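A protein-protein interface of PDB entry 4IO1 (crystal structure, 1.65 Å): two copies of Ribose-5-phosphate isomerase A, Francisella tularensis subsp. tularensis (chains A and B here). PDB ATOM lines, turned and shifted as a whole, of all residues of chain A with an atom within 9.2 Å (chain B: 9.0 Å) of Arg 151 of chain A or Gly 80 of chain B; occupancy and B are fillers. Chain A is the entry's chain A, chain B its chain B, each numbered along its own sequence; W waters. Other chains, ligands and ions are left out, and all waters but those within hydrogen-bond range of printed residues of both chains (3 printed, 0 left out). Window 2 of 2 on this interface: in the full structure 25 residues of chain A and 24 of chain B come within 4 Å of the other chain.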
ATOM      1  N   MET A 144       2.735 -15.450  13.127  1.00  0.00           N
ATOM      2  CA  MET A 144       2.840 -16.265  11.918  1.00  0.00           C
ATOM      3  C   MET A 144       3.937 -17.331  11.975  1.00  0.00           C
ATOM      4  O   MET A 144       3.868 -18.316  11.223  1.00  0.00           O
ATOM      5  CB  MET A 144       2.981 -15.422  10.636  1.00  0.00           C
ATOM      6  CG  MET A 144       4.252 -14.723  10.408  1.00  0.00           C
ATOM      7  SD  MET A 144       4.442 -14.243   8.620  1.00  0.00           S
ATOM      8  CE  MET A 144       4.538 -15.758   7.761  1.00  0.00           C
ATOM      9  N   ALA A 145       4.912 -17.159  12.872  1.00  0.00           N
ATOM     10  CA  ALA A 145       6.037 -18.071  12.974  1.00  0.00           C
ATOM     11  C   ALA A 145       5.795 -19.112  14.065  1.00  0.00           C
ATOM     12  O   ALA A 145       6.656 -19.952  14.296  1.00  0.00           O
ATOM     13  CB  ALA A 145       7.290 -17.314  13.340  1.00  0.00           C
ATOM     14  N   ARG A 146       4.655 -19.041  14.752  1.00  0.00           N
ATOM     15  CA  ARG A 146       4.434 -19.891  15.925  1.00  0.00           C
ATOM     16  C   ARG A 146       4.740 -21.394  15.690  1.00  0.00           C
ATOM     17  O   ARG A 146       5.541 -21.982  16.425  1.00  0.00           O
ATOM     18  CB  ARG A 146       3.028 -19.715  16.502  1.00  0.00           C
ATOM     19  CG  ARG A 146       2.745 -20.646  17.674  1.00  0.00           C
ATOM     20  CD  ARG A 146       1.281 -20.611  18.152  1.00  0.00           C
ATOM     21  NE  ARG A 146       0.282 -20.598  17.090  1.00  0.00           N
ATOM     22  CZ  ARG A 146      -0.193 -21.675  16.479  1.00  0.00           C
ATOM     23  NH1 ARG A 146       0.256 -22.887  16.782  1.00  0.00           N
ATOM     24  NH2 ARG A 146      -1.113 -21.534  15.539  1.00  0.00           N
ATOM     25  N   SER A 147       4.105 -21.998  14.687  1.00  0.00           N
ATOM     26  CA  SER A 147       4.303 -23.419  14.420  1.00  0.00           C
ATOM     27  C   SER A 147       5.734 -23.761  13.999  1.00  0.00           C
ATOM     28  O   SER A 147       6.300 -24.773  14.410  1.00  0.00           O
ATOM     29  CB  SER A 147       3.294 -23.895  13.364  1.00  0.00           C
ATOM     30  OG  SER A 147       1.982 -23.796  13.877  1.00  0.00           O
ATOM     31  N   TYR A 148       6.333 -22.891  13.198  1.00  0.00           N
ATOM     32  CA  TYR A 148       7.691 -23.077  12.721  1.00  0.00           C
ATOM     33  C   TYR A 148       8.649 -23.097  13.918  1.00  0.00           C
ATOM     34  O   TYR A 148       9.479 -23.975  14.052  1.00  0.00           O
ATOM     35  CB  TYR A 148       8.083 -21.964  11.718  1.00  0.00           C
ATOM     36  CG  TYR A 148       9.568 -21.893  11.533  1.00  0.00           C
ATOM     37  CD1 TYR A 148      10.260 -22.897  10.850  1.00  0.00           C
ATOM     38  CD2 TYR A 148      10.303 -20.907  12.155  1.00  0.00           C
ATOM     39  CE1 TYR A 148      11.628 -22.894  10.769  1.00  0.00           C
ATOM     40  CE2 TYR A 148      11.723 -20.872  12.042  1.00  0.00           C
ATOM     41  CZ  TYR A 148      12.358 -21.892  11.366  1.00  0.00           C
ATOM     42  OH  TYR A 148      13.738 -21.900  11.278  1.00  0.00           O
ATOM     43  N   ILE A 149       8.459 -22.145  14.843  1.00  0.00           N
ATOM     44  CA  ILE A 149       9.386 -22.034  15.946  1.00  0.00           C
ATOM     45  C   ILE A 149       9.193 -23.253  16.854  1.00  0.00           C
ATOM     46  O   ILE A 149      10.190 -23.812  17.360  1.00  0.00           O
ATOM     47  CB  ILE A 149       9.140 -20.758  16.696  1.00  0.00           C
ATOM     48  CG1 ILE A 149       9.575 -19.578  15.814  1.00  0.00           C
ATOM     49  CG2 ILE A 149       9.912 -20.738  18.035  1.00  0.00           C
ATOM     50  CD1 ILE A 149       9.176 -18.238  16.388  1.00  0.00           C
ATOM     51  N   ALA A 150       7.955 -23.655  17.079  1.00  0.00           N
ATOM     52  CA  ALA A 150       7.671 -24.862  17.897  1.00  0.00           C
ATOM     53  C   ALA A 150       8.402 -26.085  17.315  1.00  0.00           C
ATOM     54  O   ALA A 150       9.016 -26.822  18.054  1.00  0.00           O
ATOM     55  CB  ALA A 150       6.218 -25.126  18.016  1.00  0.00           C
ATOM     56  N   ARG A 151       8.386 -26.270  15.990  1.00  0.00           N
ATOM     57  CA  ARG A 151       9.146 -27.368  15.388  1.00  0.00           C
ATOM     58  C   ARG A 151      10.627 -27.241  15.702  1.00  0.00           C
ATOM     59  O   ARG A 151      11.298 -28.237  15.975  1.00  0.00           O
ATOM     60  CB  ARG A 151       8.909 -27.481  13.863  1.00  0.00           C
ATOM     61  CG  ARG A 151       7.490 -27.838  13.527  1.00  0.00           C
ATOM     62  CD  ARG A 151       7.274 -28.197  12.021  1.00  0.00           C
ATOM     63  NE  ARG A 151       7.627 -27.113  11.092  1.00  0.00           N
ATOM     64  CZ  ARG A 151       6.783 -26.152  10.695  1.00  0.00           C
ATOM     65  NH1 ARG A 151       5.551 -26.118  11.166  1.00  0.00           N
ATOM     66  NH2 ARG A 151       7.167 -25.220   9.826  1.00  0.00           N
ATOM     67  N   GLN A 152      11.169 -26.028  15.635  1.00  0.00           N
ATOM     68  CA  GLN A 152      12.577 -25.835  15.917  1.00  0.00           C
ATOM     69  C   GLN A 152      12.873 -26.125  17.374  1.00  0.00           C
ATOM     70  O   GLN A 152      13.950 -26.631  17.678  1.00  0.00           O
ATOM     71  CB  GLN A 152      13.039 -24.417  15.555  1.00  0.00           C
ATOM     72  CG  GLN A 152      12.933 -24.073  14.063  1.00  0.00           C
ATOM     73  CD  GLN A 152      13.452 -25.151  13.106  1.00  0.00           C
ATOM     74  OE1 GLN A 152      12.685 -25.826  12.427  1.00  0.00           O
ATOM     75  NE2 GLN A 152      14.734 -25.297  13.053  1.00  0.00           N
ATOM     76  N   ILE A 153      11.977 -25.722  18.281  1.00  0.00           N
ATOM     77  CA  ILE A 153      12.193 -25.995  19.712  1.00  0.00           C
ATOM     78  C   ILE A 153      12.202 -27.524  20.000  1.00  0.00           C
ATOM     79  O   ILE A 153      13.037 -28.063  20.752  1.00  0.00           O
ATOM     80  CB  ILE A 153      11.152 -25.292  20.573  1.00  0.00           C
ATOM     81  CG1 ILE A 153      11.264 -23.771  20.414  1.00  0.00           C
ATOM     82  CG2 ILE A 153      11.299 -25.720  22.034  1.00  0.00           C
ATOM     83  CD1 ILE A 153      12.574 -23.229  20.862  1.00  0.00           C
ATOM     84  N   VAL A 154      11.282 -28.247  19.379  1.00  0.00           N
ATOM     85  CA  VAL A 154      11.300 -29.697  19.466  1.00  0.00           C
ATOM     86  C   VAL A 154      12.653 -30.299  19.013  1.00  0.00           C
ATOM     87  O   VAL A 154      13.210 -31.189  19.697  1.00  0.00           O
ATOM     88  CB  VAL A 154      10.109 -30.327  18.681  1.00  0.00           C
ATOM     89  CG1 VAL A 154      10.275 -31.844  18.593  1.00  0.00           C
ATOM     90  CG2 VAL A 154       8.733 -29.962  19.346  1.00  0.00           C
ATOM     91  N   LYS A 155      13.187 -29.801  17.907  1.00  0.00           N
ATOM     92  CA  LYS A 155      14.473 -30.279  17.397  1.00  0.00           C
ATOM     93  C   LYS A 155      15.573 -30.028  18.406  1.00  0.00           C
ATOM     94  O   LYS A 155      16.508 -30.806  18.502  1.00  0.00           O
ATOM     95  CB  LYS A 155      14.828 -29.633  16.071  1.00  0.00           C
ATOM     96  CG  LYS A 155      13.962 -30.128  14.944  1.00  0.00           C
ATOM     97  CD  LYS A 155      14.362 -29.507  13.636  1.00  0.00           C
ATOM     98  CE  LYS A 155      13.446 -29.978  12.521  1.00  0.00           C
ATOM     99  NZ  LYS A 155      13.265 -28.922  11.491  1.00  0.00           N
ATOM    100  N   LEU A 156      15.453 -28.940  19.154  1.00  0.00           N
ATOM    101  CA  LEU A 156      16.420 -28.580  20.186  1.00  0.00           C
ATOM    102  C   LEU A 156      16.280 -29.398  21.453  1.00  0.00           C
ATOM    103  O   LEU A 156      17.139 -29.331  22.336  1.00  0.00           O
ATOM    104  CB  LEU A 156      16.220 -27.133  20.599  1.00  0.00           C
ATOM    105  CG  LEU A 156      16.756 -26.107  19.633  1.00  0.00           C
ATOM    106  CD1 LEU A 156      16.604 -24.762  20.257  1.00  0.00           C
ATOM    107  CD2 LEU A 156      18.211 -26.421  19.318  1.00  0.00           C
ATOM    108  N   GLY A 157      15.191 -30.142  21.570  1.00  0.00           N
ATOM    109  CA  GLY A 157      14.966 -30.971  22.734  1.00  0.00           C
ATOM    110  C   GLY A 157      14.001 -30.403  23.762  1.00  0.00           C
ATOM    111  O   GLY A 157      13.957 -30.864  24.881  1.00  0.00           O
ATOM    112  N   GLY A 158      13.218 -29.400  23.405  1.00  0.00           N
ATOM    113  CA  GLY A 158      12.237 -28.848  24.354  1.00  0.00           C
ATOM    114  C   GLY A 158      10.816 -29.197  23.925  1.00  0.00           C
ATOM    115  O   GLY A 158      10.605 -29.769  22.852  1.00  0.00           O
ATOM    116  N   GLN A 159       9.863 -28.868  24.766  1.00  0.00           N
ATOM    117  CA  GLN A 159       8.436 -29.103  24.502  1.00  0.00           C
ATOM    118  C   GLN A 159       7.747 -27.748  24.576  1.00  0.00           C
ATOM    119  O   GLN A 159       7.481 -27.239  25.655  1.00  0.00           O
ATOM    120  CB  GLN A 159       7.833 -30.072  25.551  1.00  0.00           C
ATOM    121  CG  GLN A 159       8.425 -31.440  25.536  1.00  0.00           C
ATOM    122  CD  GLN A 159       8.094 -32.160  24.248  1.00  0.00           C
ATOM    123  OE1 GLN A 159       6.960 -32.102  23.783  1.00  0.00           O
ATOM    124  NE2 GLN A 159       9.088 -32.813  23.648  1.00  0.00           N
ATOM    125  N   PRO A 160       7.434 -27.169  23.409  1.00  0.00           N
ATOM    126  CA  PRO A 160       6.853 -25.827  23.336  1.00  0.00           C
ATOM    127  C   PRO A 160       5.352 -25.922  23.563  1.00  0.00           C
ATOM    128  O   PRO A 160       4.689 -26.749  22.949  1.00  0.00           O
ATOM    129  CB  PRO A 160       7.162 -25.398  21.909  1.00  0.00           C
ATOM    130  CG  PRO A 160       7.231 -26.677  21.175  1.00  0.00           C
ATOM    131  CD  PRO A 160       7.756 -27.706  22.093  1.00  0.00           C
ATOM    132  N   LEU A 175       5.294 -18.805  23.541  1.00  0.00           N
ATOM    133  CA  LEU A 175       5.499 -20.251  23.685  1.00  0.00           C
ATOM    134  C   LEU A 175       6.299 -20.428  24.998  1.00  0.00           C
ATOM    135  O   LEU A 175       7.350 -19.839  25.175  1.00  0.00           O
ATOM    136  CB  LEU A 175       6.308 -20.850  22.532  1.00  0.00           C
ATOM    137  CG  LEU A 175       5.751 -20.811  21.122  1.00  0.00           C
ATOM    138  CD1 LEU A 175       6.752 -21.396  20.068  1.00  0.00           C
ATOM    139  CD2 LEU A 175       4.453 -21.625  21.121  1.00  0.00           C
ATOM    140  N   ILE A 195      16.677 -18.047  16.030  1.00  0.00           N
ATOM    141  CA  ILE A 195      15.490 -18.639  15.416  1.00  0.00           C
ATOM    142  C   ILE A 195      14.575 -17.577  14.845  1.00  0.00           C
ATOM    143  O   ILE A 195      14.102 -16.703  15.564  1.00  0.00           O
ATOM    144  CB  ILE A 195      14.678 -19.569  16.400  1.00  0.00           C
ATOM    145  CG1 ILE A 195      15.589 -20.641  16.968  1.00  0.00           C
ATOM    146  CG2 ILE A 195      13.525 -20.168  15.679  1.00  0.00           C
ATOM    147  CD1 ILE A 195      14.976 -21.493  18.060  1.00  0.00           C
ATOM    148  N   THR B  29       3.535 -27.584  -1.253  1.00  0.00           N
ATOM    149  CA  THR B  29       3.172 -26.349  -0.609  1.00  0.00           C
ATOM    150  C   THR B  29       4.159 -25.284  -1.105  1.00  0.00           C
ATOM    151  O   THR B  29       5.351 -25.345  -0.856  1.00  0.00           O
ATOM    152  CB  THR B  29       3.265 -26.458   0.904  1.00  0.00           C
ATOM    153  OG1 THR B  29       2.298 -27.421   1.354  1.00  0.00           O
ATOM    154  CG2 THR B  29       2.986 -25.111   1.556  1.00  0.00           C
ATOM    155  N   LEU B  30       3.629 -24.343  -1.864  1.00  0.00           N
ATOM    156  CA  LEU B  30       4.414 -23.276  -2.476  1.00  0.00           C
ATOM    157  C   LEU B  30       4.328 -22.013  -1.638  1.00  0.00           C
ATOM    158  O   LEU B  30       3.259 -21.635  -1.175  1.00  0.00           O
ATOM    159  CB  LEU B  30       3.845 -22.950  -3.862  1.00  0.00           C
ATOM    160  CG  LEU B  30       4.519 -21.803  -4.654  1.00  0.00           C
ATOM    161  CD1 LEU B  30       5.919 -22.197  -5.079  1.00  0.00           C
ATOM    162  CD2 LEU B  30       3.679 -21.492  -5.882  1.00  0.00           C
ATOM    163  N   THR B  54      -1.081 -26.159  -1.810  1.00  0.00           N
ATOM    164  CA  THR B  54      -1.284 -25.115  -0.822  1.00  0.00           C
ATOM    165  C   THR B  54      -0.389 -23.921  -1.199  1.00  0.00           C
ATOM    166  O   THR B  54       0.745 -24.123  -1.627  1.00  0.00           O
ATOM    167  CB  THR B  54      -0.863 -25.675   0.556  1.00  0.00           C
ATOM    168  OG1 THR B  54      -1.607 -26.876   0.822  1.00  0.00           O
ATOM    169  CG2 THR B  54      -1.111 -24.663   1.662  1.00  0.00           C
ATOM    170  N   VAL B  56       1.293 -20.324   0.397  1.00  0.00           N
ATOM    171  CA  VAL B  56       1.568 -19.341   1.430  1.00  0.00           C
ATOM    172  C   VAL B  56       2.160 -18.094   0.773  1.00  0.00           C
ATOM    173  O   VAL B  56       2.960 -18.193  -0.159  1.00  0.00           O
ATOM    174  CB  VAL B  56       2.566 -19.904   2.468  1.00  0.00           C
ATOM    175  CG1 VAL B  56       2.902 -18.883   3.546  1.00  0.00           C
ATOM    176  CG2 VAL B  56       1.984 -21.172   3.133  1.00  0.00           C
ATOM    177  N   VAL B  74      -3.103 -19.593   2.262  1.00  0.00           N
ATOM    178  CA  VAL B  74      -3.314 -20.075   3.617  1.00  0.00           C
ATOM    179  C   VAL B  74      -2.221 -19.524   4.534  1.00  0.00           C
ATOM    180  O   VAL B  74      -1.131 -19.224   4.077  1.00  0.00           O
ATOM    181  CB  VAL B  74      -3.255 -21.631   3.682  1.00  0.00           C
ATOM    182  CG1 VAL B  74      -4.355 -22.260   2.766  1.00  0.00           C
ATOM    183  CG2 VAL B  74      -1.920 -22.143   3.332  1.00  0.00           C
ATOM    184  N   ASP B  75      -2.563 -19.374   5.809  1.00  0.00           N
ATOM    185  CA  ASP B  75      -1.627 -18.937   6.832  1.00  0.00           C
ATOM    186  C   ASP B  75      -0.566 -20.000   7.044  1.00  0.00           C
ATOM    187  O   ASP B  75      -0.849 -21.187   7.050  1.00  0.00           O
ATOM    188  CB  ASP B  75      -2.429 -18.692   8.114  1.00  0.00           C
ATOM    189  CG  ASP B  75      -1.572 -18.257   9.297  1.00  0.00           C
ATOM    190  OD1 ASP B  75      -1.354 -17.037   9.478  1.00  0.00           O
ATOM    191  OD2 ASP B  75      -1.145 -19.135  10.076  1.00  0.00           O
ATOM    192  N   LEU B  76       0.672 -19.567   7.293  1.00  0.00           N
ATOM    193  CA  LEU B  76       1.770 -20.512   7.478  1.00  0.00           C
ATOM    194  C   LEU B  76       1.539 -21.516   8.585  1.00  0.00           C
ATOM    195  O   LEU B  76       1.944 -22.662   8.482  1.00  0.00           O
ATOM    196  CB  LEU B  76       3.089 -19.744   7.704  1.00  0.00           C
ATOM    197  CG  LEU B  76       4.355 -20.593   7.861  1.00  0.00           C
ATOM    198  CD1 LEU B  76       4.622 -21.479   6.637  1.00  0.00           C
ATOM    199  CD2 LEU B  76       5.528 -19.683   8.149  1.00  0.00           C
ATOM    200  N   ASN B  77       0.907 -21.100   9.685  1.00  0.00           N
ATOM    201  CA  ASN B  77       0.650 -22.036  10.769  1.00  0.00           C
ATOM    202  C   ASN B  77      -0.247 -23.200  10.336  1.00  0.00           C
ATOM    203  O   ASN B  77      -0.116 -24.318  10.828  1.00  0.00           O
ATOM    204  CB  ASN B  77       0.014 -21.304  11.951  1.00  0.00           C
ATOM    205  CG  ASN B  77       0.983 -20.373  12.652  1.00  0.00           C
ATOM    206  OD1 ASN B  77       2.073 -20.811  13.078  1.00  0.00           O
ATOM    207  ND2 ASN B  77       0.567 -19.120  12.844  1.00  0.00           N
ATOM    208  N   TYR B  78      -1.153 -22.926   9.413  1.00  0.00           N
ATOM    209  CA  TYR B  78      -2.036 -23.972   8.902  1.00  0.00           C
ATOM    210  C   TYR B  78      -1.346 -24.805   7.822  1.00  0.00           C
ATOM    211  O   TYR B  78      -1.573 -26.006   7.729  1.00  0.00           O
ATOM    212  CB  TYR B  78      -3.337 -23.354   8.384  1.00  0.00           C
ATOM    213  CG  TYR B  78      -4.276 -22.906   9.485  1.00  0.00           C
ATOM    214  CD1 TYR B  78      -4.437 -23.674  10.636  1.00  0.00           C
ATOM    215  CD2 TYR B  78      -5.030 -21.741   9.360  1.00  0.00           C
ATOM    216  CE1 TYR B  78      -5.299 -23.285  11.645  1.00  0.00           C
ATOM    217  CE2 TYR B  78      -5.900 -21.345  10.365  1.00  0.00           C
ATOM    218  CZ  TYR B  78      -6.028 -22.126  11.507  1.00  0.00           C
ATOM    219  OH  TYR B  78      -6.886 -21.752  12.518  1.00  0.00           O
ATOM    220  N   ALA B  79      -0.472 -24.187   7.037  1.00  0.00           N
ATOM    221  CA  ALA B  79       0.201 -24.890   5.943  1.00  0.00           C
ATOM    222  C   ALA B  79       1.269 -25.876   6.392  1.00  0.00           C
ATOM    223  O   ALA B  79       1.489 -26.907   5.751  1.00  0.00           O
ATOM    224  CB  ALA B  79       0.782 -23.911   5.001  1.00  0.00           C
ATOM    225  N   GLY B  80       1.945 -25.566   7.492  1.00  0.00           N
ATOM    226  CA  GLY B  80       3.074 -26.368   7.909  1.00  0.00           C
ATOM    227  C   GLY B  80       4.314 -25.956   7.131  1.00  0.00           C
ATOM    228  O   GLY B  80       4.551 -24.783   6.911  1.00  0.00           O
ATOM    229  N   GLU B  81       5.094 -26.929   6.702  1.00  0.00           N
ATOM    230  CA  GLU B  81       6.368 -26.661   6.084  1.00  0.00           C
ATOM    231  C   GLU B  81       6.131 -26.223   4.644  1.00  0.00           C
ATOM    232  O   GLU B  81       5.243 -26.766   3.980  1.00  0.00           O
ATOM    233  CB  GLU B  81       7.209 -27.920   6.086  1.00  0.00           C
ATOM    234  CG  GLU B  81       8.686 -27.702   6.327  1.00  0.00           C
ATOM    235  CD  GLU B  81       9.405 -28.989   6.714  1.00  0.00           C
ATOM    236  OE1 GLU B  81       8.717 -29.969   7.086  1.00  0.00           O
ATOM    237  OE2 GLU B  81      10.656 -29.013   6.646  1.00  0.00           O
ATOM    238  N   ILE B  82       6.919 -25.259   4.172  1.00  0.00           N
ATOM    239  CA  ILE B  82       6.913 -24.878   2.761  1.00  0.00           C
ATOM    240  C   ILE B  82       7.923 -25.771   2.010  1.00  0.00           C
ATOM    241  O   ILE B  82       9.070 -25.942   2.463  1.00  0.00           O
ATOM    242  CB  ILE B  82       7.240 -23.362   2.590  1.00  0.00           C
ATOM    243  CG1 ILE B  82       6.179 -22.467   3.235  1.00  0.00           C
ATOM    244  CG2 ILE B  82       7.399 -22.992   1.097  1.00  0.00           C
ATOM    245  CD1 ILE B  82       6.569 -20.999   3.291  1.00  0.00           C
ATOM    246  N   ASP B  83       7.488 -26.386   0.906  1.00  0.00           N
ATOM    247  CA  ASP B  83       8.393 -27.164   0.068  1.00  0.00           C
ATOM    248  C   ASP B  83       9.308 -26.260  -0.767  1.00  0.00           C
ATOM    249  O   ASP B  83      10.517 -26.485  -0.871  1.00  0.00           O
ATOM    250  CB  ASP B  83       7.587 -28.056  -0.850  1.00  0.00           C
ATOM    251  CG  ASP B  83       6.840 -29.156  -0.077  1.00  0.00           C
ATOM    252  OD1 ASP B  83       7.524 -29.982   0.562  1.00  0.00           O
ATOM    253  OD2 ASP B  83       5.599 -29.173  -0.079  1.00  0.00           O
ATOM    254  N   ILE B 111      10.578 -15.406   7.682  1.00  0.00           N
ATOM    255  CA  ILE B 111       9.918 -16.579   8.240  1.00  0.00           C
ATOM    256  C   ILE B 111       9.609 -17.623   7.172  1.00  0.00           C
ATOM    257  O   ILE B 111       9.804 -18.839   7.370  1.00  0.00           O
ATOM    258  CB  ILE B 111       8.664 -16.194   9.040  1.00  0.00           C
ATOM    259  CG1 ILE B 111       9.050 -15.315  10.217  1.00  0.00           C
ATOM    260  CG2 ILE B 111       7.897 -17.437   9.448  1.00  0.00           C
ATOM    261  CD1 ILE B 111       7.913 -14.611  10.905  1.00  0.00           C
ATOM    262  N   CYS B 112       9.106 -17.165   6.038  1.00  0.00           N
ATOM    263  CA  CYS B 112       8.793 -18.069   4.942  1.00  0.00           C
ATOM    264  C   CYS B 112      10.043 -18.800   4.460  1.00  0.00           C
ATOM    265  O   CYS B 112      10.023 -20.032   4.296  1.00  0.00           O
ATOM    266  CB  CYS B 112       8.156 -17.356   3.772  1.00  0.00           C
ATOM    267  SG  CYS B 112       6.393 -16.946   4.071  1.00  0.00           S
ATOM    268  N   ALA B 114      12.662 -19.348   6.272  1.00  0.00           N
ATOM    269  CA  ALA B 114      13.066 -20.224   7.365  1.00  0.00           C
ATOM    270  C   ALA B 114      12.298 -21.550   7.303  1.00  0.00           C
ATOM    271  O   ALA B 114      12.874 -22.616   7.603  1.00  0.00           O
ATOM    272  CB  ALA B 114      12.847 -19.537   8.700  1.00  0.00           C
ATOM    273  N   ALA B 115      11.006 -21.477   6.941  1.00  0.00           N
ATOM    274  CA  ALA B 115      10.124 -22.630   6.960  1.00  0.00           C
ATOM    275  C   ALA B 115      10.154 -23.433   5.662  1.00  0.00           C
ATOM    276  O   ALA B 115       9.441 -24.440   5.563  1.00  0.00           O
ATOM    277  CB  ALA B 115       8.694 -22.189   7.218  1.00  0.00           C
ATOM    278  N   ALA B 116      10.941 -22.955   4.687  1.00  0.00           N
ATOM    279  CA  ALA B 116      11.065 -23.558   3.371  1.00  0.00           C
ATOM    280  C   ALA B 116      12.169 -24.611   3.223  1.00  0.00           C
ATOM    281  O   ALA B 116      13.335 -24.367   3.576  1.00  0.00           O
ATOM    282  CB  ALA B 116      11.274 -22.487   2.349  1.00  0.00           C
ATOM    283  N   LYS B 117      11.827 -25.744   2.631  1.00  0.00           N
ATOM    284  CA  LYS B 117      12.812 -26.769   2.339  1.00  0.00           C
ATOM    285  C   LYS B 117      13.784 -26.282   1.265  1.00  0.00           C
ATOM    286  O   LYS B 117      14.963 -26.574   1.329  1.00  0.00           O
ATOM    287  CB  LYS B 117      12.155 -28.077   1.901  1.00  0.00           C
ATOM    288  CG  LYS B 117      11.337 -28.737   2.986  1.00  0.00           C
ATOM    289  CD  LYS B 117      10.690 -30.032   2.459  1.00  0.00           C
ATOM    290  CE  LYS B 117       9.867 -30.732   3.516  1.00  0.00           C
ATOM    291  NZ  LYS B 117       8.840 -31.610   2.887  1.00  0.00           N
HETATM  292  O   HOH W   1       4.977 -23.604   9.770  1.00  0.00           O
HETATM  293  O   HOH W   2      14.795 -23.292   9.271  1.00  0.00           O
HETATM  294  O   HOH W   3       4.568 -20.954  11.482  1.00  0.00           O
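Hydrophobic or aromatic side chains of chain B that line the printed part of chain A: Leu 76, Ile 111 and Ala 114.
Of the 19 printed residues of chain A, 6 touch a printed residue of chain B.
Among the printed residues, no Asp or Glu carboxylate lies within 4 Å of a Lys or Arg side-chain nitrogen of the other chain.
N of Ile 82 of chain B is in hydrogen-bond range of O of Ala 115 of chain B, at 3.0 Å.
The guanidinium group of Arg 146 of chain A lies within hydrogen-bond range of the side-chain hydroxyl of Ser 147 of chain A (3.5 Å).
OD2 of Asp 75 of chain B lies within hydrogen-bond range of N of Asn 77 of chain B (2.9 Å).
The backbone NH (N) of Ser 147 of chain A is in hydrogen-bond range of the side-chain amide oxygen (OD1) of Asn 77 of chain B (2.9 Å).
Among the printed residues, merely in contact across the chains: Met 144 of chain A with Leu 76 of chain B, Met 144 of chain A with Asn 77 of chain B, Met 144 of chain A with Ile 111 of chain B, Ala 145 of chain A with Ile 111 of chain B, Arg 146 of chain A with Asn 77 of chain B, Tyr 148 of chain A with Ala 114 of chain B, Tyr 148 of chain A with Ala 115 of chain B and Arg 151 of chain A with Gly 80 of chain B.
Of chain B, only Gly 80 comes within 4 Å of Arg 151 of chain A.
Gly 80 of chain B touches just one residue of chain A: Arg 151.
No residue of chain A comes within 4 Å of Ala 79 of chain B.
Of the printed residues of chain A, Leu 76 of chain B touches Met 144 (3.8 Å).
Of the printed residues of chain B, Ser 147 of chain A touches Asn 77 (2.9 Å).
Of the printed residues of chain B, Met 144 of chain A touches Leu 76, Asn 77 and Ile 111.
Of the printed residues of chain A, Ala 115 of chain B touches Tyr 148 (3.9 Å).
Printed residues of chain A within 4 Å of Ala 114 of chain B: Tyr 148 (3.4 Å).
Val 154 of chain A touches none of the printed residues of chain B.
The nearest residue of chain B that does not touch Arg 151 of chain A is Glu 81 of chain B (4.1 Å).
The nearest printed residue of chain A that does not touch Gly 80 of chain B is Ser 147 of chain A (6.0 Å).
The nearest printed residue of chain B that does not touch Met 144 of chain A is Cys 112 of chain B (4.3 Å).
No position is printed for both chains.
Water W2 bridges O of Ala 114 of chain B (2.6 Å) and OH of Tyr 148 of chain A (2.7 Å).
Water W1 lies within hydrogen-bond range of the guanidinium group of Arg 151 of chain A (2.7 Å), the backbone carbonyl oxygen of Gly 80 of chain B (3.1 Å) and the backbone carbonyl oxygen of Leu 76 of chain B (3.4 Å).
Water W3 lies within hydrogen-bond range of the backbone carbonyl oxygen (O) of Met 144 of chain A, the side-chain amide oxygen (OD1) of Asn 77 of chain B, the backbone NH (N) of Tyr 148 of chain A and the backbone NH (N) of Ser 147 of chain A.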
